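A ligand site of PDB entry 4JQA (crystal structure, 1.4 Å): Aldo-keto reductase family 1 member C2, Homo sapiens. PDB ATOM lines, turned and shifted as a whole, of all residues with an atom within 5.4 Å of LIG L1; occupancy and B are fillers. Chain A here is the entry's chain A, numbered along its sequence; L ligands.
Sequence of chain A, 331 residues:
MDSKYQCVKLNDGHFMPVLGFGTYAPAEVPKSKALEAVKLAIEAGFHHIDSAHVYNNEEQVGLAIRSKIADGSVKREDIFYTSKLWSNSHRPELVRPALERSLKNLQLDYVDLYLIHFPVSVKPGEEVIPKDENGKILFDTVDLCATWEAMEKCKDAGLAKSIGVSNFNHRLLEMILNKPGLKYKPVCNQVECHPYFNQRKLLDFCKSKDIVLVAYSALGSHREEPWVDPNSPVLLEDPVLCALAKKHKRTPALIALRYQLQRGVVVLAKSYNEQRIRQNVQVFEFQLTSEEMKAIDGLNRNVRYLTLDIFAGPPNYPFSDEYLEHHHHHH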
ATOM      1  N   TYR A  24     -20.794 -25.520   0.970  1.00  0.00           N
ATOM      2  CA  TYR A  24     -21.213 -25.799  -0.405  1.00  0.00           C
ATOM      3  C   TYR A  24     -21.608 -27.254  -0.548  1.00  0.00           C
ATOM      4  O   TYR A  24     -20.876 -28.118  -0.025  1.00  0.00           O
ATOM      5  CB  TYR A  24     -20.092 -25.562  -1.429  1.00  0.00           C
ATOM      6  CG  TYR A  24     -20.523 -25.986  -2.823  1.00  0.00           C
ATOM      7  CD1 TYR A  24     -21.454 -25.247  -3.503  1.00  0.00           C
ATOM      8  CD2 TYR A  24     -20.085 -27.184  -3.371  1.00  0.00           C
ATOM      9  CE1 TYR A  24     -21.888 -25.627  -4.752  1.00  0.00           C
ATOM     10  CE2 TYR A  24     -20.548 -27.584  -4.605  1.00  0.00           C
ATOM     11  CZ  TYR A  24     -21.457 -26.815  -5.279  1.00  0.00           C
ATOM     12  OH  TYR A  24     -21.951 -27.225  -6.518  1.00  0.00           O
ATOM     13  N   VAL A  54     -22.777 -17.505  -4.319  1.00  0.00           N
ATOM     14  CA  VAL A  54     -22.960 -18.473  -5.361  1.00  0.00           C
ATOM     15  C   VAL A  54     -23.363 -19.892  -4.866  1.00  0.00           C
ATOM     16  O   VAL A  54     -23.774 -20.693  -5.617  1.00  0.00           O
ATOM     17  CB  VAL A  54     -21.703 -18.401  -6.228  1.00  0.00           C
ATOM     18  CG1 VAL A  54     -20.562 -19.245  -5.723  1.00  0.00           C
ATOM     19  CG2 VAL A  54     -21.961 -18.354  -7.692  1.00  0.00           C
ATOM     20  N   TYR A  55     -23.246 -20.139  -3.591  1.00  0.00           N
ATOM     21  CA  TYR A  55     -23.696 -21.381  -2.998  1.00  0.00           C
ATOM     22  C   TYR A  55     -25.203 -21.510  -2.868  1.00  0.00           C
ATOM     23  O   TYR A  55     -25.675 -22.593  -2.551  1.00  0.00           O
ATOM     24  CB  TYR A  55     -23.040 -21.668  -1.646  1.00  0.00           C
ATOM     25  CG  TYR A  55     -21.494 -21.672  -1.688  1.00  0.00           C
ATOM     26  CD1 TYR A  55     -20.803 -21.766  -2.887  1.00  0.00           C
ATOM     27  CD2 TYR A  55     -20.732 -21.686  -0.516  1.00  0.00           C
ATOM     28  CE1 TYR A  55     -19.435 -21.723  -2.930  1.00  0.00           C
ATOM     29  CE2 TYR A  55     -19.371 -21.665  -0.554  1.00  0.00           C
ATOM     30  CZ  TYR A  55     -18.691 -21.691  -1.764  1.00  0.00           C
ATOM     31  OH  TYR A  55     -17.296 -21.619  -1.788  1.00  0.00           O
ATOM     32  N   LYS A  84     -18.632 -14.226   0.144  1.00  0.00           N
ATOM     33  CA  LYS A  84     -17.772 -13.988  -0.973  1.00  0.00           C
ATOM     34  C   LYS A  84     -18.553 -13.202  -2.027  1.00  0.00           C
ATOM     35  O   LYS A  84     -19.708 -13.543  -2.297  1.00  0.00           O
ATOM     36  CB  LYS A  84     -17.150 -15.294  -1.584  1.00  0.00           C
ATOM     37  CG  LYS A  84     -16.499 -16.193  -0.532  1.00  0.00           C
ATOM     38  CD  LYS A  84     -15.795 -17.409  -1.148  1.00  0.00           C
ATOM     39  CE  LYS A  84     -15.437 -18.465  -0.118  1.00  0.00           C
ATOM     40  NZ  LYS A  84     -16.533 -19.391   0.169  1.00  0.00           N
ATOM     41  N   TRP A  86     -19.264 -12.470  -5.630  1.00  0.00           N
ATOM     42  CA  TRP A  86     -19.232 -13.195  -6.911  1.00  0.00           C
ATOM     43  C   TRP A  86     -18.825 -12.221  -8.048  1.00  0.00           C
ATOM     44  O   TRP A  86     -18.890 -11.023  -7.956  1.00  0.00           O
ATOM     45  CB  TRP A  86     -20.578 -13.932  -7.190  1.00  0.00           C
ATOM     46  CG  TRP A  86     -20.401 -14.792  -8.422  1.00  0.00           C
ATOM     47  CD1 TRP A  86     -21.076 -14.677  -9.561  1.00  0.00           C
ATOM     48  CD2 TRP A  86     -19.417 -15.800  -8.609  1.00  0.00           C
ATOM     49  NE1 TRP A  86     -20.571 -15.540 -10.477  1.00  0.00           N
ATOM     50  CE2 TRP A  86     -19.538 -16.234  -9.917  1.00  0.00           C
ATOM     51  CE3 TRP A  86     -18.400 -16.347  -7.805  1.00  0.00           C
ATOM     52  CZ2 TRP A  86     -18.693 -17.201 -10.451  1.00  0.00           C
ATOM     53  CZ3 TRP A  86     -17.544 -17.294  -8.332  1.00  0.00           C
ATOM     54  CH2 TRP A  86     -17.710 -17.720  -9.674  1.00  0.00           C
ATOM     55  N   HIS A 117     -14.248 -13.592  -4.606  1.00  0.00           N
ATOM     56  CA  HIS A 117     -14.341 -15.053  -4.785  1.00  0.00           C
ATOM     57  C   HIS A 117     -13.385 -15.617  -5.832  1.00  0.00           C
ATOM     58  O   HIS A 117     -12.753 -16.691  -5.642  1.00  0.00           O
ATOM     59  CB  HIS A 117     -15.779 -15.469  -5.125  1.00  0.00           C
ATOM     60  CG  HIS A 117     -16.126 -16.879  -4.809  1.00  0.00           C
ATOM     61  ND1 HIS A 117     -17.402 -17.246  -4.501  1.00  0.00           N
ATOM     62  CD2 HIS A 117     -15.386 -18.034  -4.738  1.00  0.00           C
ATOM     63  CE1 HIS A 117     -17.495 -18.528  -4.295  1.00  0.00           C
ATOM     64  NE2 HIS A 117     -16.275 -19.035  -4.438  1.00  0.00           N
ATOM     65  N   PHE A 118     -13.271 -14.871  -6.944  1.00  0.00           N
ATOM     66  CA  PHE A 118     -12.569 -15.385  -8.108  1.00  0.00           C
ATOM     67  C   PHE A 118     -12.183 -14.222  -9.006  1.00  0.00           C
ATOM     68  O   PHE A 118     -12.975 -13.321  -9.190  1.00  0.00           O
ATOM     69  CB  PHE A 118     -13.426 -16.368  -8.868  1.00  0.00           C
ATOM     70  CG  PHE A 118     -12.655 -17.151  -9.918  1.00  0.00           C
ATOM     71  CD1 PHE A 118     -11.776 -18.132  -9.545  1.00  0.00           C
ATOM     72  CD2 PHE A 118     -12.801 -16.915 -11.292  1.00  0.00           C
ATOM     73  CE1 PHE A 118     -11.017 -18.861 -10.483  1.00  0.00           C
ATOM     74  CE2 PHE A 118     -12.061 -17.653 -12.217  1.00  0.00           C
ATOM     75  CZ  PHE A 118     -11.165 -18.586 -11.825  1.00  0.00           C
ATOM     76  N   VAL A 128     -25.422 -15.728 -12.311  1.00  0.00           N
ATOM     77  CA  VAL A 128     -24.093 -15.907 -11.839  1.00  0.00           C
ATOM     78  C   VAL A 128     -23.061 -16.409 -12.905  1.00  0.00           C
ATOM     79  O   VAL A 128     -21.908 -16.002 -12.822  1.00  0.00           O
ATOM     80  CB  VAL A 128     -23.989 -16.816 -10.597  1.00  0.00           C
ATOM     81  CG1 VAL A 128     -24.691 -16.081  -9.391  1.00  0.00           C
ATOM     82  CG2 VAL A 128     -24.498 -18.245 -10.781  1.00  0.00           C
ATOM     83  N   ILE A 129     -23.492 -17.202 -13.872  1.00  0.00           N
ATOM     84  CA  ILE A 129     -22.610 -17.480 -15.020  1.00  0.00           C
ATOM     85  C   ILE A 129     -23.382 -17.039 -16.288  1.00  0.00           C
ATOM     86  O   ILE A 129     -24.084 -17.861 -16.944  1.00  0.00           O
ATOM     87  CB  ILE A 129     -22.239 -18.969 -15.080  1.00  0.00           C
ATOM     88  CG1 ILE A 129     -21.450 -19.329 -13.777  1.00  0.00           C
ATOM     89  CG2 ILE A 129     -21.386 -19.253 -16.311  1.00  0.00           C
ATOM     90  CD1 ILE A 129     -21.060 -20.783 -13.719  1.00  0.00           C
ATOM     91  N   ASN A 167      -8.535 -17.609  -4.620  1.00  0.00           N
ATOM     92  CA  ASN A 167      -8.123 -18.031  -5.971  1.00  0.00           C
ATOM     93  C   ASN A 167      -7.168 -17.041  -6.598  1.00  0.00           C
ATOM     94  O   ASN A 167      -7.180 -16.868  -7.863  1.00  0.00           O
ATOM     95  CB  ASN A 167      -9.321 -18.370  -6.849  1.00  0.00           C
ATOM     96  CG  ASN A 167     -10.129 -19.478  -6.224  1.00  0.00           C
ATOM     97  OD1 ASN A 167      -9.600 -20.618  -6.123  1.00  0.00           O
ATOM     98  ND2 ASN A 167     -11.386 -19.231  -5.896  1.00  0.00           N
ATOM     99  N   TRP A 227     -17.171 -30.094 -12.410  1.00  0.00           N
ATOM    100  CA  TRP A 227     -16.121 -29.238 -11.862  1.00  0.00           C
ATOM    101  C   TRP A 227     -14.767 -29.996 -11.679  1.00  0.00           C
ATOM    102  O   TRP A 227     -13.676 -29.417 -11.806  1.00  0.00           O
ATOM    103  CB  TRP A 227     -16.595 -28.625 -10.529  1.00  0.00           C
ATOM    104  CG  TRP A 227     -17.830 -27.858 -10.627  1.00  0.00           C
ATOM    105  CD1 TRP A 227     -19.069 -28.278 -10.300  1.00  0.00           C
ATOM    106  CD2 TRP A 227     -17.962 -26.469 -11.028  1.00  0.00           C
ATOM    107  NE1 TRP A 227     -19.995 -27.251 -10.525  1.00  0.00           N
ATOM    108  CE2 TRP A 227     -19.329 -26.145 -10.966  1.00  0.00           C
ATOM    109  CE3 TRP A 227     -17.048 -25.481 -11.466  1.00  0.00           C
ATOM    110  CZ2 TRP A 227     -19.813 -24.859 -11.319  1.00  0.00           C
ATOM    111  CZ3 TRP A 227     -17.511 -24.224 -11.812  1.00  0.00           C
ATOM    112  CH2 TRP A 227     -18.890 -23.916 -11.741  1.00  0.00           C
ATOM    113  N   LEU A 306      -9.830 -28.512  -8.713  1.00  0.00           N
ATOM    114  CA  LEU A 306     -10.752 -27.474  -9.172  1.00  0.00           C
ATOM    115  C   LEU A 306     -10.013 -26.483 -10.069  1.00  0.00           C
ATOM    116  O   LEU A 306      -9.361 -25.562  -9.629  1.00  0.00           O
ATOM    117  CB  LEU A 306     -11.362 -26.783  -7.976  1.00  0.00           C
ATOM    118  CG  LEU A 306     -12.724 -26.133  -8.282  1.00  0.00           C
ATOM    119  CD1 LEU A 306     -13.755 -27.222  -8.631  1.00  0.00           C
ATOM    120  CD2 LEU A 306     -13.200 -25.267  -7.110  1.00  0.00           C
ATOM    121  N   LEU A 308     -11.490 -24.824 -12.538  1.00  0.00           N
ATOM    122  CA  LEU A 308     -12.384 -23.734 -12.849  1.00  0.00           C
ATOM    123  C   LEU A 308     -12.134 -23.316 -14.311  1.00  0.00           C
ATOM    124  O   LEU A 308     -12.229 -22.131 -14.632  1.00  0.00           O
ATOM    125  CB  LEU A 308     -12.142 -22.542 -11.852  1.00  0.00           C
ATOM    126  CG  LEU A 308     -12.404 -22.980 -10.398  1.00  0.00           C
ATOM    127  CD1 LEU A 308     -11.914 -22.048  -9.307  1.00  0.00           C
ATOM    128  CD2 LEU A 308     -13.887 -23.298 -10.235  1.00  0.00           C
ATOM    129  N   PHE A 311     -13.724 -20.686 -16.843  1.00  0.00           N
ATOM    130  CA  PHE A 311     -13.295 -19.301 -16.776  1.00  0.00           C
ATOM    131  C   PHE A 311     -11.852 -18.997 -17.317  1.00  0.00           C
ATOM    132  O   PHE A 311     -11.351 -17.875 -17.144  1.00  0.00           O
ATOM    133  CB  PHE A 311     -13.422 -18.753 -15.338  1.00  0.00           C
ATOM    134  CG  PHE A 311     -14.778 -18.922 -14.748  1.00  0.00           C
ATOM    135  CD1 PHE A 311     -15.804 -18.078 -15.082  1.00  0.00           C
ATOM    136  CD2 PHE A 311     -14.953 -19.854 -13.707  1.00  0.00           C
ATOM    137  CE1 PHE A 311     -17.054 -18.186 -14.515  1.00  0.00           C
ATOM    138  CE2 PHE A 311     -16.184 -19.983 -13.099  1.00  0.00           C
ATOM    139  CZ  PHE A 311     -17.243 -19.148 -13.491  1.00  0.00           C
HETATM  140  O1  LIG L   1     -16.451 -21.686  -4.449  1.00  0.00           O
HETATM  141  C1  LIG L   1     -16.896 -22.205  -5.482  1.00  0.00           C
HETATM  142  O2  LIG L   1     -17.638 -23.244  -5.441  1.00  0.00           O
HETATM  143  C2  LIG L   1     -16.557 -21.613  -6.739  1.00  0.00           C
HETATM  144  C3  LIG L   1     -15.257 -21.008  -6.846  1.00  0.00           C
HETATM  145  C4  LIG L   1     -14.767 -20.374  -8.048  1.00  0.00           C
HETATM  146  C5  LIG L   1     -15.588 -20.434  -9.180  1.00  0.00           C
HETATM  147  C6  LIG L   1     -16.866 -20.980  -9.068  1.00  0.00           C
HETATM  148  C7  LIG L   1     -17.393 -21.575  -7.913  1.00  0.00           C
HETATM  149  N1  LIG L   1     -18.621 -22.109  -7.844  1.00  0.00           N
HETATM  150  C8  LIG L   1     -19.754 -21.712  -8.515  1.00  0.00           C
HETATM  151  C9  LIG L   1     -20.804 -22.650  -8.509  1.00  0.00           C
HETATM  152  C10 LIG L   1     -20.637 -23.814  -7.822  1.00  0.00           C
HETATM  153  C11 LIG L   1     -19.899 -20.517  -9.196  1.00  0.00           C
HETATM  154  C12 LIG L   1     -21.119 -20.267  -9.871  1.00  0.00           C
HETATM  155  C13 LIG L   1     -22.139 -21.187  -9.827  1.00  0.00           C
HETATM  156  C14 LIG L   1     -22.025 -22.391  -9.150  1.00  0.00           C
HETATM  157  C15 LIG L   1     -23.155 -23.261  -9.205  1.00  0.00           C
HETATM  158  P1  LG2 L   2     -13.992 -30.893   1.219  1.00  0.00           P
HETATM  159  O1  LG2 L   2     -12.682 -31.152   0.694  1.00  0.00           O
HETATM  160  O2  LG2 L   2     -14.089 -30.296   2.546  1.00  0.00           O
HETATM  161  O3  LG2 L   2     -14.684 -32.300   1.243  1.00  0.00           O
HETATM  162  C1  LG2 L   2     -16.069 -32.534   1.360  1.00  0.00           C
HETATM  163  C2  LG2 L   2     -16.290 -34.011   1.169  1.00  0.00           C
HETATM  164  O4  LG2 L   2     -15.556 -34.804   2.162  1.00  0.00           O
HETATM  165  C3  LG2 L   2     -17.816 -34.276   1.080  1.00  0.00           C
HETATM  166  O5  LG2 L   2     -18.111 -35.393   0.147  1.00  0.00           O
HETATM  167  C4  LG2 L   2     -17.954 -34.779   2.530  1.00  0.00           C
HETATM  168  O6  LG2 L   2     -19.036 -35.712   2.653  1.00  0.00           O
HETATM  169  C5  LG2 L   2     -16.593 -35.488   2.839  1.00  0.00           C
HETATM  170  N1  LG2 L   2     -16.131 -35.592   4.235  1.00  0.00           N
HETATM  171  C6  LG2 L   2     -16.189 -34.642   5.147  1.00  0.00           C
HETATM  172  N2  LG2 L   2     -15.659 -35.080   6.275  1.00  0.00           N
HETATM  173  C7  LG2 L   2     -15.246 -36.350   6.105  1.00  0.00           C
HETATM  174  C8  LG2 L   2     -14.615 -37.280   6.908  1.00  0.00           C
HETATM  175  N3  LG2 L   2     -14.364 -37.044   8.180  1.00  0.00           N
HETATM  176  N4  LG2 L   2     -14.345 -38.549   6.478  1.00  0.00           N
HETATM  177  C9  LG2 L   2     -14.658 -38.775   5.196  1.00  0.00           C
HETATM  178  N5  LG2 L   2     -15.254 -37.890   4.298  1.00  0.00           N
HETATM  179  C10 LG2 L   2     -15.511 -36.631   4.790  1.00  0.00           C
HETATM  180  O7  LG2 L   2     -15.078 -30.177   0.200  1.00  0.00           O
HETATM  181  P2  LG2 L   2     -15.073 -28.805  -0.607  1.00  0.00           P
HETATM  182  O8  LG2 L   2     -14.321 -28.954  -1.820  1.00  0.00           O
HETATM  183  O9  LG2 L   2     -16.521 -28.612  -0.493  1.00  0.00           O
HETATM  184  O10 LG2 L   2     -14.280 -27.726   0.217  1.00  0.00           O
HETATM  185  C11 LG2 L   2     -14.873 -27.348   1.500  1.00  0.00           C
HETATM  186  C12 LG2 L   2     -15.404 -25.906   1.429  1.00  0.00           C
HETATM  187  O11 LG2 L   2     -14.462 -24.947   0.932  1.00  0.00           O
HETATM  188  C13 LG2 L   2     -16.704 -25.748   0.594  1.00  0.00           C
HETATM  189  O12 LG2 L   2     -17.859 -26.304   1.224  1.00  0.00           O
HETATM  190  C14 LG2 L   2     -16.730 -24.209   0.465  1.00  0.00           C
HETATM  191  O13 LG2 L   2     -17.165 -23.665   1.750  1.00  0.00           O
HETATM  192  C15 LG2 L   2     -15.234 -23.938   0.278  1.00  0.00           C
HETATM  193  N6  LG2 L   2     -14.762 -23.839  -1.106  1.00  0.00           N
HETATM  194  C16 LG2 L   2     -14.327 -22.643  -1.594  1.00  0.00           C
HETATM  195  C17 LG2 L   2     -13.926 -22.447  -2.903  1.00  0.00           C
HETATM  196  C18 LG2 L   2     -13.407 -21.197  -3.359  1.00  0.00           C
HETATM  197  O14 LG2 L   2     -13.209 -20.949  -4.563  1.00  0.00           O
HETATM  198  N7  LG2 L   2     -13.072 -20.293  -2.475  1.00  0.00           N
HETATM  199  C19 LG2 L   2     -13.936 -23.599  -3.698  1.00  0.00           C
HETATM  200  C20 LG2 L   2     -14.324 -24.820  -3.244  1.00  0.00           C
HETATM  201  C21 LG2 L   2     -14.726 -24.962  -1.930  1.00  0.00           C
HETATM  202  P3  LG2 L   2     -20.181 -35.583   3.714  1.00  0.00           P
HETATM  203  O15 LG2 L   2     -20.776 -34.187   3.502  1.00  0.00           O
HETATM  204  O16 LG2 L   2     -21.063 -36.711   3.308  1.00  0.00           O
HETATM  205  O17 LG2 L   2     -19.486 -35.879   5.016  1.00  0.00           O
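A ring nitrogen (NE2) of His 117 lies within hydrogen-bond range of an oxygen (O1) of LIG L1 (2.7 Å). OH of Tyr 55 is in hydrogen-bond range of O1 of LIG L1 (2.8 Å). The side-chain amide nitrogen (ND2) of Asn 167 is in hydrogen-bond range of an oxygen (O14) of LG2 L2 (2.8 Å). An oxygen (O12) of LG2 L2 is in hydrogen-bond range of the backbone NH (N) of Tyr 24, at 3.0 Å.
The side-chain hydroxyl (OH) of Tyr 55 is in hydrogen-bond range of the side-chain amino group (NZ) of Lys 84 (3.1 Å). The backbone carbonyl oxygen (O) of His 117 lies within hydrogen-bond range of the side-chain amide nitrogen (ND2) of Asn 167 (2.9 Å). NE1 of Trp 86 lies within hydrogen-bond range of O of Val 128 (2.7 Å).
Merely in contact with LIG L1: Val 54, Trp 86, Leu 308, Trp 227, Tyr 24, Ile 129, Val 128 and Phe 311. Hydrophobic or aromatic side chains within 4 Å of LIG L1: Tyr 24, Val 54, Tyr 55, Trp 86, His 117, Val 128, Ile 129, Trp 227, Leu 308 and Phe 311. The nearest printed residue that does not touch LIG L1 is Phe 118 (4.03 Å).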
